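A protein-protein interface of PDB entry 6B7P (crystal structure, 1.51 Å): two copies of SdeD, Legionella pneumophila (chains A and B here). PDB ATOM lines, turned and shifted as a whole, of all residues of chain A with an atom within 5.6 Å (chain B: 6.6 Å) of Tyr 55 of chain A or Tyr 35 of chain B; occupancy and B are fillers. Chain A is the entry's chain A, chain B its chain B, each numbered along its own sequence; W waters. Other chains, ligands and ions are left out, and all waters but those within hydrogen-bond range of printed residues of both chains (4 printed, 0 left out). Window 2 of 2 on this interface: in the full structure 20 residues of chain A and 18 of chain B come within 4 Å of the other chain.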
ATOM      1  N   GLN A  53      27.361  -0.490  -4.127  1.00  0.00           N
ATOM      2  CA  GLN A  53      26.663  -0.098  -2.915  1.00  0.00           C
ATOM      3  C   GLN A  53      26.569   1.448  -2.755  1.00  0.00           C
ATOM      4  O   GLN A  53      26.848   2.030  -1.706  1.00  0.00           O
ATOM      5  CB  GLN A  53      27.346  -0.678  -1.686  1.00  0.00           C
ATOM      6  CG  GLN A  53      27.573  -2.211  -1.861  1.00  0.00           C
ATOM      7  CD  GLN A  53      26.626  -2.948  -1.063  1.00  0.00           C
ATOM      8  OE1 GLN A  53      25.504  -3.222  -1.497  1.00  0.00           O
ATOM      9  NE2 GLN A  53      27.047  -3.298   0.138  1.00  0.00           N
ATOM     10  N   ARG A  54      26.080   2.088  -3.823  1.00  0.00           N
ATOM     11  CA  ARG A  54      25.945   3.524  -3.795  1.00  0.00           C
ATOM     12  C   ARG A  54      24.933   3.954  -2.855  1.00  0.00           C
ATOM     13  O   ARG A  54      25.046   4.996  -2.164  1.00  0.00           O
ATOM     14  CB  ARG A  54      25.603   4.007  -5.200  1.00  0.00           C
ATOM     15  CG  ARG A  54      26.694   3.911  -6.236  1.00  0.00           C
ATOM     16  CD  ARG A  54      26.145   4.143  -7.644  1.00  0.00           C
ATOM     17  NE  ARG A  54      25.213   3.050  -7.981  1.00  0.00           N
ATOM     18  CZ  ARG A  54      23.999   3.192  -8.550  1.00  0.00           C
ATOM     19  NH1 ARG A  54      23.598   4.383  -8.899  1.00  0.00           N
ATOM     20  NH2 ARG A  54      23.266   2.121  -8.768  1.00  0.00           N
ATOM     21  N   TYR A  55      23.870   3.189  -2.724  1.00  0.00           N
ATOM     22  CA  TYR A  55      22.740   3.468  -1.847  1.00  0.00           C
ATOM     23  C   TYR A  55      21.918   2.203  -1.694  1.00  0.00           C
ATOM     24  O   TYR A  55      22.068   1.321  -2.469  1.00  0.00           O
ATOM     25  CB  TYR A  55      21.831   4.609  -2.363  1.00  0.00           C
ATOM     26  CG  TYR A  55      21.136   4.321  -3.669  1.00  0.00           C
ATOM     27  CD1 TYR A  55      19.978   3.601  -3.707  1.00  0.00           C
ATOM     28  CD2 TYR A  55      21.647   4.758  -4.827  1.00  0.00           C
ATOM     29  CE1 TYR A  55      19.341   3.312  -4.903  1.00  0.00           C
ATOM     30  CE2 TYR A  55      21.029   4.488  -6.024  1.00  0.00           C
ATOM     31  CZ  TYR A  55      19.858   3.760  -6.048  1.00  0.00           C
ATOM     32  OH  TYR A  55      19.205   3.489  -7.254  1.00  0.00           O
ATOM     33  N   ILE A  56      21.068   2.153  -0.680  1.00  0.00           N
ATOM     34  CA  ILE A  56      20.063   1.107  -0.567  1.00  0.00           C
ATOM     35  C   ILE A  56      18.761   1.836  -0.363  1.00  0.00           C
ATOM     36  O   ILE A  56      18.637   2.792   0.334  1.00  0.00           O
ATOM     37  CB  ILE A  56      20.355   0.040   0.522  1.00  0.00           C
ATOM     38  CG1 ILE A  56      19.325  -1.075   0.564  1.00  0.00           C
ATOM     39  CG2 ILE A  56      20.446   0.735   1.841  1.00  0.00           C
ATOM     40  CD1 ILE A  56      19.751  -2.241   1.406  1.00  0.00           C
ATOM     41  N   THR A  57      17.642   1.353  -0.938  1.00  0.00           N
ATOM     42  CA  THR A  57      16.370   1.951  -0.736  1.00  0.00           C
ATOM     43  C   THR A  57      15.560   1.130   0.267  1.00  0.00           C
ATOM     44  O   THR A  57      15.445  -0.098   0.127  1.00  0.00           O
ATOM     45  CB  THR A  57      15.590   2.000  -2.085  1.00  0.00           C
ATOM     46  OG1 THR A  57      16.373   2.751  -2.997  1.00  0.00           O
ATOM     47  CG2 THR A  57      14.261   2.694  -1.880  1.00  0.00           C
ATOM     48  N   GLN A  62      15.926   6.472  -0.131  1.00  0.00           N
ATOM     49  CA  GLN A  62      17.316   6.107  -0.479  1.00  0.00           C
ATOM     50  C   GLN A  62      18.205   6.458   0.709  1.00  0.00           C
ATOM     51  O   GLN A  62      18.325   7.630   1.058  1.00  0.00           O
ATOM     52  CB  GLN A  62      17.822   6.776  -1.735  1.00  0.00           C
ATOM     53  CG  GLN A  62      16.987   6.246  -2.931  1.00  0.00           C
ATOM     54  CD  GLN A  62      17.600   6.654  -4.257  1.00  0.00           C
ATOM     55  OE1 GLN A  62      18.479   7.527  -4.370  1.00  0.00           O
ATOM     56  NE2 GLN A  62      17.176   5.899  -5.315  1.00  0.00           N
ATOM     57  N   LEU A  63      18.903   5.441   1.156  1.00  0.00           N
ATOM     58  CA  LEU A  63      19.933   5.582   2.216  1.00  0.00           C
ATOM     59  C   LEU A  63      21.253   5.540   1.522  1.00  0.00           C
ATOM     60  O   LEU A  63      21.715   4.494   1.007  1.00  0.00           O
ATOM     61  CB  LEU A  63      19.851   4.447   3.234  1.00  0.00           C
ATOM     62  CG  LEU A  63      20.931   4.461   4.357  1.00  0.00           C
ATOM     63  CD1 LEU A  63      20.770   5.628   5.186  1.00  0.00           C
ATOM     64  CD2 LEU A  63      20.770   3.205   5.136  1.00  0.00           C
ATOM     65  N   HIS A  64      21.860   6.713   1.367  1.00  0.00           N
ATOM     66  CA  HIS A  64      23.080   6.871   0.619  1.00  0.00           C
ATOM     67  C   HIS A  64      24.282   6.259   1.377  1.00  0.00           C
ATOM     68  O   HIS A  64      24.249   6.188   2.640  1.00  0.00           O
ATOM     69  CB  HIS A  64      23.368   8.280   0.228  1.00  0.00           C
ATOM     70  CG  HIS A  64      22.446   8.744  -0.858  1.00  0.00           C
ATOM     71  ND1 HIS A  64      22.529   8.237  -2.109  1.00  0.00           N
ATOM     72  CD2 HIS A  64      21.312   9.510  -0.808  1.00  0.00           C
ATOM     73  CE1 HIS A  64      21.464   8.644  -2.829  1.00  0.00           C
ATOM     74  NE2 HIS A  64      20.714   9.408  -2.052  1.00  0.00           N
ATOM     75  N   ARG A  65      25.285   5.793   0.654  1.00  0.00           N
ATOM     76  CA  ARG A  65      26.594   5.348   1.214  1.00  0.00           C
ATOM     77  C   ARG A  65      26.392   4.427   2.393  1.00  0.00           C
ATOM     78  O   ARG A  65      27.010   4.598   3.459  1.00  0.00           O
ATOM     79  CB  ARG A  65      27.509   6.552   1.490  1.00  0.00           C
ATOM     80  CG  ARG A  65      27.028   7.560   2.484  1.00  0.00           C
ATOM     81  CD  ARG A  65      28.095   8.639   2.730  1.00  0.00           C
ATOM     82  NE  ARG A  65      28.049   9.675   1.734  1.00  0.00           N
ATOM     83  CZ  ARG A  65      29.042  10.384   1.279  1.00  0.00           C
ATOM     84  NH1 ARG A  65      30.269  10.221   1.754  1.00  0.00           N
ATOM     85  NH2 ARG A  65      28.870  11.265   0.261  1.00  0.00           N
ATOM     86  N   PRO A  66      25.593   3.345   2.304  1.00  0.00           N
ATOM     87  CA  PRO A  66      25.265   2.525   3.466  1.00  0.00           C
ATOM     88  C   PRO A  66      26.440   1.865   4.119  1.00  0.00           C
ATOM     89  O   PRO A  66      26.324   1.560   5.321  1.00  0.00           O
ATOM     90  CB  PRO A  66      24.319   1.448   2.856  1.00  0.00           C
ATOM     91  CG  PRO A  66      24.575   1.475   1.354  1.00  0.00           C
ATOM     92  CD  PRO A  66      24.861   2.914   1.087  1.00  0.00           C
ATOM     93  N   SER B  31      10.763   4.597  -7.755  1.00  0.00           N
ATOM     94  CA  SER B  31      11.364   3.300  -7.879  1.00  0.00           C
ATOM     95  C   SER B  31      11.454   2.819  -9.307  1.00  0.00           C
ATOM     96  O   SER B  31      12.354   2.120  -9.638  1.00  0.00           O
ATOM     97  CB  SER B  31      10.652   2.276  -7.013  1.00  0.00           C
ATOM     98  OG  SER B  31       9.319   2.283  -7.279  1.00  0.00           O
ATOM     99  N   TRP B  33      12.467   4.405 -11.707  1.00  0.00           N
ATOM    100  CA  TRP B  33      13.618   5.093 -12.349  1.00  0.00           C
ATOM    101  C   TRP B  33      14.984   4.833 -11.660  1.00  0.00           C
ATOM    102  O   TRP B  33      15.934   5.519 -11.948  1.00  0.00           O
ATOM    103  CB  TRP B  33      13.327   6.589 -12.402  1.00  0.00           C
ATOM    104  CG  TRP B  33      12.288   6.923 -13.468  1.00  0.00           C
ATOM    105  CD1 TRP B  33      10.949   7.129 -13.261  1.00  0.00           C
ATOM    106  CD2 TRP B  33      12.582   7.141 -14.870  1.00  0.00           C
ATOM    107  NE1 TRP B  33      10.375   7.439 -14.509  1.00  0.00           N
ATOM    108  CE2 TRP B  33      11.320   7.441 -15.490  1.00  0.00           C
ATOM    109  CE3 TRP B  33      13.737   7.092 -15.644  1.00  0.00           C
ATOM    110  CZ2 TRP B  33      11.298   7.727 -16.866  1.00  0.00           C
ATOM    111  CZ3 TRP B  33      13.699   7.380 -16.996  1.00  0.00           C
ATOM    112  CH2 TRP B  33      12.442   7.675 -17.573  1.00  0.00           C
ATOM    113  N   GLU B  34      15.059   3.808 -10.829  1.00  0.00           N
ATOM    114  CA  GLU B  34      16.325   3.360 -10.234  1.00  0.00           C
ATOM    115  C   GLU B  34      17.144   2.530 -11.217  1.00  0.00           C
ATOM    116  O   GLU B  34      16.620   1.959 -12.108  1.00  0.00           O
ATOM    117  CB  GLU B  34      16.077   2.584  -8.940  1.00  0.00           C
ATOM    118  CG  GLU B  34      15.677   3.496  -7.794  1.00  0.00           C
ATOM    119  CD  GLU B  34      15.500   2.814  -6.450  1.00  0.00           C
ATOM    120  OE1 GLU B  34      15.394   1.593  -6.411  1.00  0.00           O
ATOM    121  OE2 GLU B  34      15.442   3.539  -5.466  1.00  0.00           O
ATOM    122  N   TYR B  35      18.438   2.481 -11.038  1.00  0.00           N
ATOM    123  CA  TYR B  35      19.324   1.812 -11.946  1.00  0.00           C
ATOM    124  C   TYR B  35      20.396   1.053 -11.186  1.00  0.00           C
ATOM    125  O   TYR B  35      20.798   1.472 -10.181  1.00  0.00           O
ATOM    126  CB  TYR B  35      19.986   2.822 -12.889  1.00  0.00           C
ATOM    127  CG  TYR B  35      20.700   2.209 -14.042  1.00  0.00           C
ATOM    128  CD1 TYR B  35      20.004   1.737 -15.116  1.00  0.00           C
ATOM    129  CD2 TYR B  35      22.059   2.133 -14.069  1.00  0.00           C
ATOM    130  CE1 TYR B  35      20.643   1.163 -16.166  1.00  0.00           C
ATOM    131  CE2 TYR B  35      22.692   1.558 -15.106  1.00  0.00           C
ATOM    132  CZ  TYR B  35      21.968   1.095 -16.163  1.00  0.00           C
ATOM    133  OH  TYR B  35      22.585   0.530 -17.212  1.00  0.00           O
ATOM    134  N   ASN B  36      20.838  -0.056 -11.743  1.00  0.00           N
ATOM    135  CA  ASN B  36      21.814  -0.964 -11.146  1.00  0.00           C
ATOM    136  C   ASN B  36      22.857  -1.292 -12.215  1.00  0.00           C
ATOM    137  O   ASN B  36      22.513  -1.761 -13.211  1.00  0.00           O
ATOM    138  CB  ASN B  36      21.042  -2.217 -10.648  1.00  0.00           C
ATOM    139  CG  ASN B  36      21.925  -3.402 -10.282  1.00  0.00           C
ATOM    140  OD1 ASN B  36      23.122  -3.414 -10.469  1.00  0.00           O
ATOM    141  ND2 ASN B  36      21.282  -4.427  -9.752  1.00  0.00           N
ATOM    142  N   TYR B  37      24.117  -1.008 -11.980  1.00  0.00           N
ATOM    143  CA  TYR B  37      25.212  -1.220 -12.966  1.00  0.00           C
ATOM    144  C   TYR B  37      25.680  -2.691 -13.007  1.00  0.00           C
ATOM    145  O   TYR B  37      26.170  -3.083 -14.044  1.00  0.00           O
ATOM    146  CB  TYR B  37      26.455  -0.323 -12.660  1.00  0.00           C
ATOM    147  CG  TYR B  37      26.148   1.120 -12.897  1.00  0.00           C
ATOM    148  CD1 TYR B  37      25.633   1.903 -11.899  1.00  0.00           C
ATOM    149  CD2 TYR B  37      26.386   1.696 -14.152  1.00  0.00           C
ATOM    150  CE1 TYR B  37      25.368   3.230 -12.136  1.00  0.00           C
ATOM    151  CE2 TYR B  37      26.073   3.007 -14.408  1.00  0.00           C
ATOM    152  CZ  TYR B  37      25.569   3.758 -13.371  1.00  0.00           C
ATOM    153  OH  TYR B  37      25.252   5.086 -13.601  1.00  0.00           O
ATOM    154  N   LYS B  38      25.502  -3.420 -11.898  1.00  0.00           N
ATOM    155  CA  LYS B  38      26.007  -4.808 -11.723  1.00  0.00           C
ATOM    156  C   LYS B  38      25.053  -5.809 -12.370  1.00  0.00           C
ATOM    157  O   LYS B  38      25.496  -6.741 -13.069  1.00  0.00           O
ATOM    158  CB  LYS B  38      26.189  -5.130 -10.209  1.00  0.00           C
ATOM    159  CG  LYS B  38      27.305  -6.135  -9.832  1.00  0.00           C
ATOM    160  CD  LYS B  38      27.779  -5.993  -8.361  1.00  0.00           C
ATOM    161  CE  LYS B  38      26.823  -6.632  -7.336  1.00  0.00           C
ATOM    162  NZ  LYS B  38      26.781  -8.130  -7.406  1.00  0.00           N
ATOM    163  N   ASN B  39      23.750  -5.610 -12.145  1.00  0.00           N
ATOM    164  CA  ASN B  39      22.687  -6.528 -12.644  1.00  0.00           C
ATOM    165  C   ASN B  39      21.583  -5.726 -13.334  1.00  0.00           C
ATOM    166  O   ASN B  39      20.937  -4.931 -12.667  1.00  0.00           O
ATOM    167  CB  ASN B  39      22.047  -7.343 -11.480  1.00  0.00           C
ATOM    168  CG  ASN B  39      23.077  -7.836 -10.460  1.00  0.00           C
ATOM    169  OD1 ASN B  39      23.395  -7.147  -9.476  1.00  0.00           O
ATOM    170  ND2 ASN B  39      23.627  -9.022 -10.705  1.00  0.00           N
ATOM    171  N   PRO B  40      21.328  -5.952 -14.646  1.00  0.00           N
ATOM    172  CA  PRO B  40      20.123  -5.301 -15.203  1.00  0.00           C
ATOM    173  C   PRO B  40      18.864  -5.598 -14.366  1.00  0.00           C
ATOM    174  O   PRO B  40      18.774  -6.619 -13.708  1.00  0.00           O
ATOM    175  CB  PRO B  40      19.962  -5.920 -16.606  1.00  0.00           C
ATOM    176  CG  PRO B  40      21.223  -6.691 -16.894  1.00  0.00           C
ATOM    177  CD  PRO B  40      21.950  -6.912 -15.586  1.00  0.00           C
ATOM    178  N   THR B  41      17.896  -4.699 -14.397  1.00  0.00           N
ATOM    179  CA  THR B  41      16.675  -4.885 -13.670  1.00  0.00           C
ATOM    180  C   THR B  41      15.610  -4.214 -14.493  1.00  0.00           C
ATOM    181  O   THR B  41      15.917  -3.421 -15.421  1.00  0.00           O
ATOM    182  CB  THR B  41      16.664  -4.168 -12.297  1.00  0.00           C
ATOM    183  OG1 THR B  41      17.016  -2.757 -12.483  1.00  0.00           O
ATOM    184  CG2 THR B  41      17.567  -4.860 -11.336  1.00  0.00           C
ATOM    185  N   THR B  43      13.291  -1.305 -15.125  1.00  0.00           N
ATOM    186  CA  THR B  43      13.324   0.108 -14.834  1.00  0.00           C
ATOM    187  C   THR B  43      13.097   0.836 -16.180  1.00  0.00           C
ATOM    188  O   THR B  43      13.424   0.327 -17.250  1.00  0.00           O
ATOM    189  CB  THR B  43      14.783   0.459 -14.314  1.00  0.00           C
ATOM    190  OG1 THR B  43      14.782   1.865 -14.011  1.00  0.00           O
ATOM    191  CG2 THR B  43      15.881   0.173 -15.271  1.00  0.00           C
ATOM    192  N   ALA B  45      14.894   3.717 -16.352  1.00  0.00           N
ATOM    193  CA  ALA B  45      16.137   4.440 -16.443  1.00  0.00           C
ATOM    194  C   ALA B  45      17.121   3.758 -17.343  1.00  0.00           C
ATOM    195  O   ALA B  45      17.070   2.513 -17.538  1.00  0.00           O
ATOM    196  CB  ALA B  45      16.725   4.554 -15.093  1.00  0.00           C
ATOM    197  N   LYS B  46      18.081   4.528 -17.887  1.00  0.00           N
ATOM    198  CA  LYS B  46      19.189   3.942 -18.629  1.00  0.00           C
ATOM    199  C   LYS B  46      20.540   4.377 -17.973  1.00  0.00           C
ATOM    200  O   LYS B  46      21.619   4.273 -18.584  1.00  0.00           O
ATOM    201  CB  LYS B  46      19.092   4.348 -20.075  1.00  0.00           C
ATOM    202  CG  LYS B  46      17.843   3.827 -20.754  1.00  0.00           C
ATOM    203  CD  LYS B  46      17.913   4.302 -22.231  1.00  0.00           C
ATOM    204  CE  LYS B  46      17.030   3.470 -23.148  1.00  0.00           C
ATOM    205  NZ  LYS B  46      15.731   3.340 -22.467  1.00  0.00           N
ATOM    206  N   GLY B  47      20.460   4.862 -16.768  1.00  0.00           N
ATOM    207  CA  GLY B  47      21.603   5.253 -16.042  1.00  0.00           C
ATOM    208  C   GLY B  47      21.184   5.823 -14.694  1.00  0.00           C
ATOM    209  O   GLY B  47      19.999   5.740 -14.301  1.00  0.00           O
ATOM    210  N   ASP B  48      22.106   6.383 -13.914  1.00  0.00           N
ATOM    211  CA  ASP B  48      21.876   6.854 -12.590  1.00  0.00           C
ATOM    212  C   ASP B  48      21.365   8.263 -12.483  1.00  0.00           C
ATOM    213  O   ASP B  48      21.148   8.978 -13.468  1.00  0.00           O
ATOM    214  CB  ASP B  48      23.206   6.732 -11.770  1.00  0.00           C
ATOM    215  CG  ASP B  48      24.140   7.814 -12.008  1.00  0.00           C
ATOM    216  OD1 ASP B  48      24.213   8.260 -13.154  1.00  0.00           O
ATOM    217  OD2 ASP B  48      24.875   8.100 -11.008  1.00  0.00           O
ATOM    218  N   GLY B  49      21.076   8.700 -11.278  1.00  0.00           N
ATOM    219  CA  GLY B  49      20.798  10.078 -11.005  1.00  0.00           C
ATOM    220  C   GLY B  49      19.338  10.551 -10.800  1.00  0.00           C
ATOM    221  O   GLY B  49      19.034  11.645 -10.389  1.00  0.00           O
ATOM    222  N   HIS B  50      18.396   9.652 -11.197  1.00  0.00           N
ATOM    223  CA  HIS B  50      17.042  10.085 -11.265  1.00  0.00           C
ATOM    224  C   HIS B  50      16.420  10.530  -9.985  1.00  0.00           C
ATOM    225  O   HIS B  50      15.567  11.357  -9.896  1.00  0.00           O
ATOM    226  CB  HIS B  50      16.091   9.003 -11.920  1.00  0.00           C
ATOM    227  CG  HIS B  50      16.256   8.887 -13.402  1.00  0.00           C
ATOM    228  ND1 HIS B  50      15.522   9.670 -14.266  1.00  0.00           N
ATOM    229  CD2 HIS B  50      17.122   8.202 -14.188  1.00  0.00           C
ATOM    230  CE1 HIS B  50      15.931   9.410 -15.493  1.00  0.00           C
ATOM    231  NE2 HIS B  50      16.897   8.538 -15.475  1.00  0.00           N
ATOM    232  N   ASN B  51      16.857   9.887  -8.893  1.00  0.00           N
ATOM    233  CA  ASN B  51      16.251  10.200  -7.576  1.00  0.00           C
ATOM    234  C   ASN B  51      17.159  11.107  -6.675  1.00  0.00           C
ATOM    235  O   ASN B  51      16.796  11.258  -5.471  1.00  0.00           O
ATOM    236  CB  ASN B  51      15.900   8.903  -6.835  1.00  0.00           C
ATOM    237  CG  ASN B  51      14.688   8.256  -7.505  1.00  0.00           C
ATOM    238  OD1 ASN B  51      13.661   8.873  -7.397  1.00  0.00           O
ATOM    239  ND2 ASN B  51      14.841   7.140  -8.076  1.00  0.00           N
ATOM    240  N   LEU B  52      18.146  11.718  -7.296  1.00  0.00           N
ATOM    241  CA  LEU B  52      19.063  12.634  -6.488  1.00  0.00           C
ATOM    242  C   LEU B  52      18.505  14.005  -6.442  1.00  0.00           C
ATOM    243  O   LEU B  52      17.987  14.555  -7.394  1.00  0.00           O
ATOM    244  CB  LEU B  52      20.407  12.640  -7.153  1.00  0.00           C
ATOM    245  CG  LEU B  52      21.052  11.282  -7.113  1.00  0.00           C
ATOM    246  CD1 LEU B  52      22.500  11.374  -7.591  1.00  0.00           C
ATOM    247  CD2 LEU B  52      20.970  10.450  -5.787  1.00  0.00           C
ATOM    248  N   TYR B 130      23.332  11.230 -17.431  1.00  0.00           N
ATOM    249  CA  TYR B 130      23.882  10.384 -18.449  1.00  0.00           C
ATOM    250  C   TYR B 130      23.325  10.746 -19.798  1.00  0.00           C
ATOM    251  O   TYR B 130      22.310  11.411 -19.881  1.00  0.00           O
ATOM    252  CB  TYR B 130      23.630   8.895 -18.057  1.00  0.00           C
ATOM    253  CG  TYR B 130      22.168   8.513 -17.941  1.00  0.00           C
ATOM    254  CD1 TYR B 130      21.448   8.133 -19.030  1.00  0.00           C
ATOM    255  CD2 TYR B 130      21.483   8.589 -16.722  1.00  0.00           C
ATOM    256  CE1 TYR B 130      20.172   7.752 -18.932  1.00  0.00           C
ATOM    257  CE2 TYR B 130      20.113   8.281 -16.568  1.00  0.00           C
ATOM    258  CZ  TYR B 130      19.435   7.851 -17.729  1.00  0.00           C
ATOM    259  OH  TYR B 130      18.138   7.510 -17.551  1.00  0.00           O
HETATM  260  O   HOH W   1      20.426   4.891  -9.692  1.00  0.00           O
HETATM  261  O   HOH W   2      19.232   8.179  -7.546  1.00  0.00           O
HETATM  262  O   HOH W   3      24.209   7.382  -8.123  1.00  0.00           O
HETATM  263  O   HOH W   4      19.919   0.694  -7.425  1.00  0.00           O
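NH2 of Arg 54 of chain A lies within hydrogen-bond range of O of Tyr 35 of chain B (2.9 Å). The side-chain hydroxyl of Thr 57 of chain A is in hydrogen-bond range of the side-chain carboxylate of Glu 34 of chain B (2.8 Å). OE2 of Glu 34 of chain B sits at hydrogen-bond distance from NE2 of Gln 62 of chain A (2.9 Å).
O of Arg 54 of chain A sits at hydrogen-bond distance from N of Arg 65 of chain A (2.9 Å). OG1 of Thr 43 of chain B sits at hydrogen-bond distance from O of Glu 34 of chain B (2.6 Å). OD1 of Asp 48 of chain B sits close to OH of Tyr 37 of chain B.
Arg 54 of chain A touches Tyr 37 of chain B. Asp 48 of chain B touches Arg 54 of chain A. OH of Tyr 55 of chain A touches CG of Glu 34 of chain B, at 3.6 Å. O of Tyr 35 of chain B touches OH of Tyr 55 of chain A, at 3.9 Å. Asn 51 of chain B touches Gln 62 of chain A (CB to NE2, 3.6 Å). CD2 of Leu 52 of chain B touches CE1 of His 64 of chain A, 3.5 Å away.
Printed residues of chain B within 4 Å of Tyr 55 of chain A: Glu 34 and Tyr 35. Ile 56 of chain A touches none of the printed residues of chain B. Tyr 35 of chain B touches just these residues of chain A: Arg 54 (2.9 Å) and Tyr 55 (3.9 Å). Of the printed residues of chain A, Asp 48 of chain B touches Arg 54. Of the printed residues of chain A, Asn 51 of chain B touches Gln 62.
Of the 10 printed residues of chain A, 5 touch a printed residue of chain B. Hydrophobic or aromatic side chains of chain A within 4 Å of the printed part of chain B: Tyr 55 and His 64. Of the 20 printed residues of chain B, 6 touch a printed residue of chain A. Printed residues of chain B that touch a printed residue of chain A: Glu 34, Tyr 35, Tyr 37, Asp 48, Asn 51 and Leu 52. Hydrophobic or aromatic side chains of chain B within 4 Å of the printed part of chain A: Tyr 37 and Leu 52.
No position is printed for both chains. Of the 9 pairs that touch across the chains among the printed residues, none has its exchanged pair printed and touching as well.
Water W4 bridges OH of Tyr 55 of chain A (2.9 Å) and O of Tyr 35 of chain B (3.0 Å). Water W3 lies within hydrogen-bond range of the side-chain carboxylate of Asp 48 of chain B (3.0 Å) and the guanidinium group of Arg 54 of chain A (3.2 Å). Water W1 lies within hydrogen-bond range of the side-chain hydroxyl (OH) of Tyr 55 of chain A (3.1 Å), the guanidinium group (NH1) of Arg 54 of chain A (3.3 Å) and the backbone NH (N) of Tyr 35 of chain B (3.4 Å). Water W2 lies within hydrogen-bond range of the backbone NH of Asn 51 of chain B (3.2 Å) and the side-chain amide oxygen of Gln 62 of chain A (3.3 Å).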
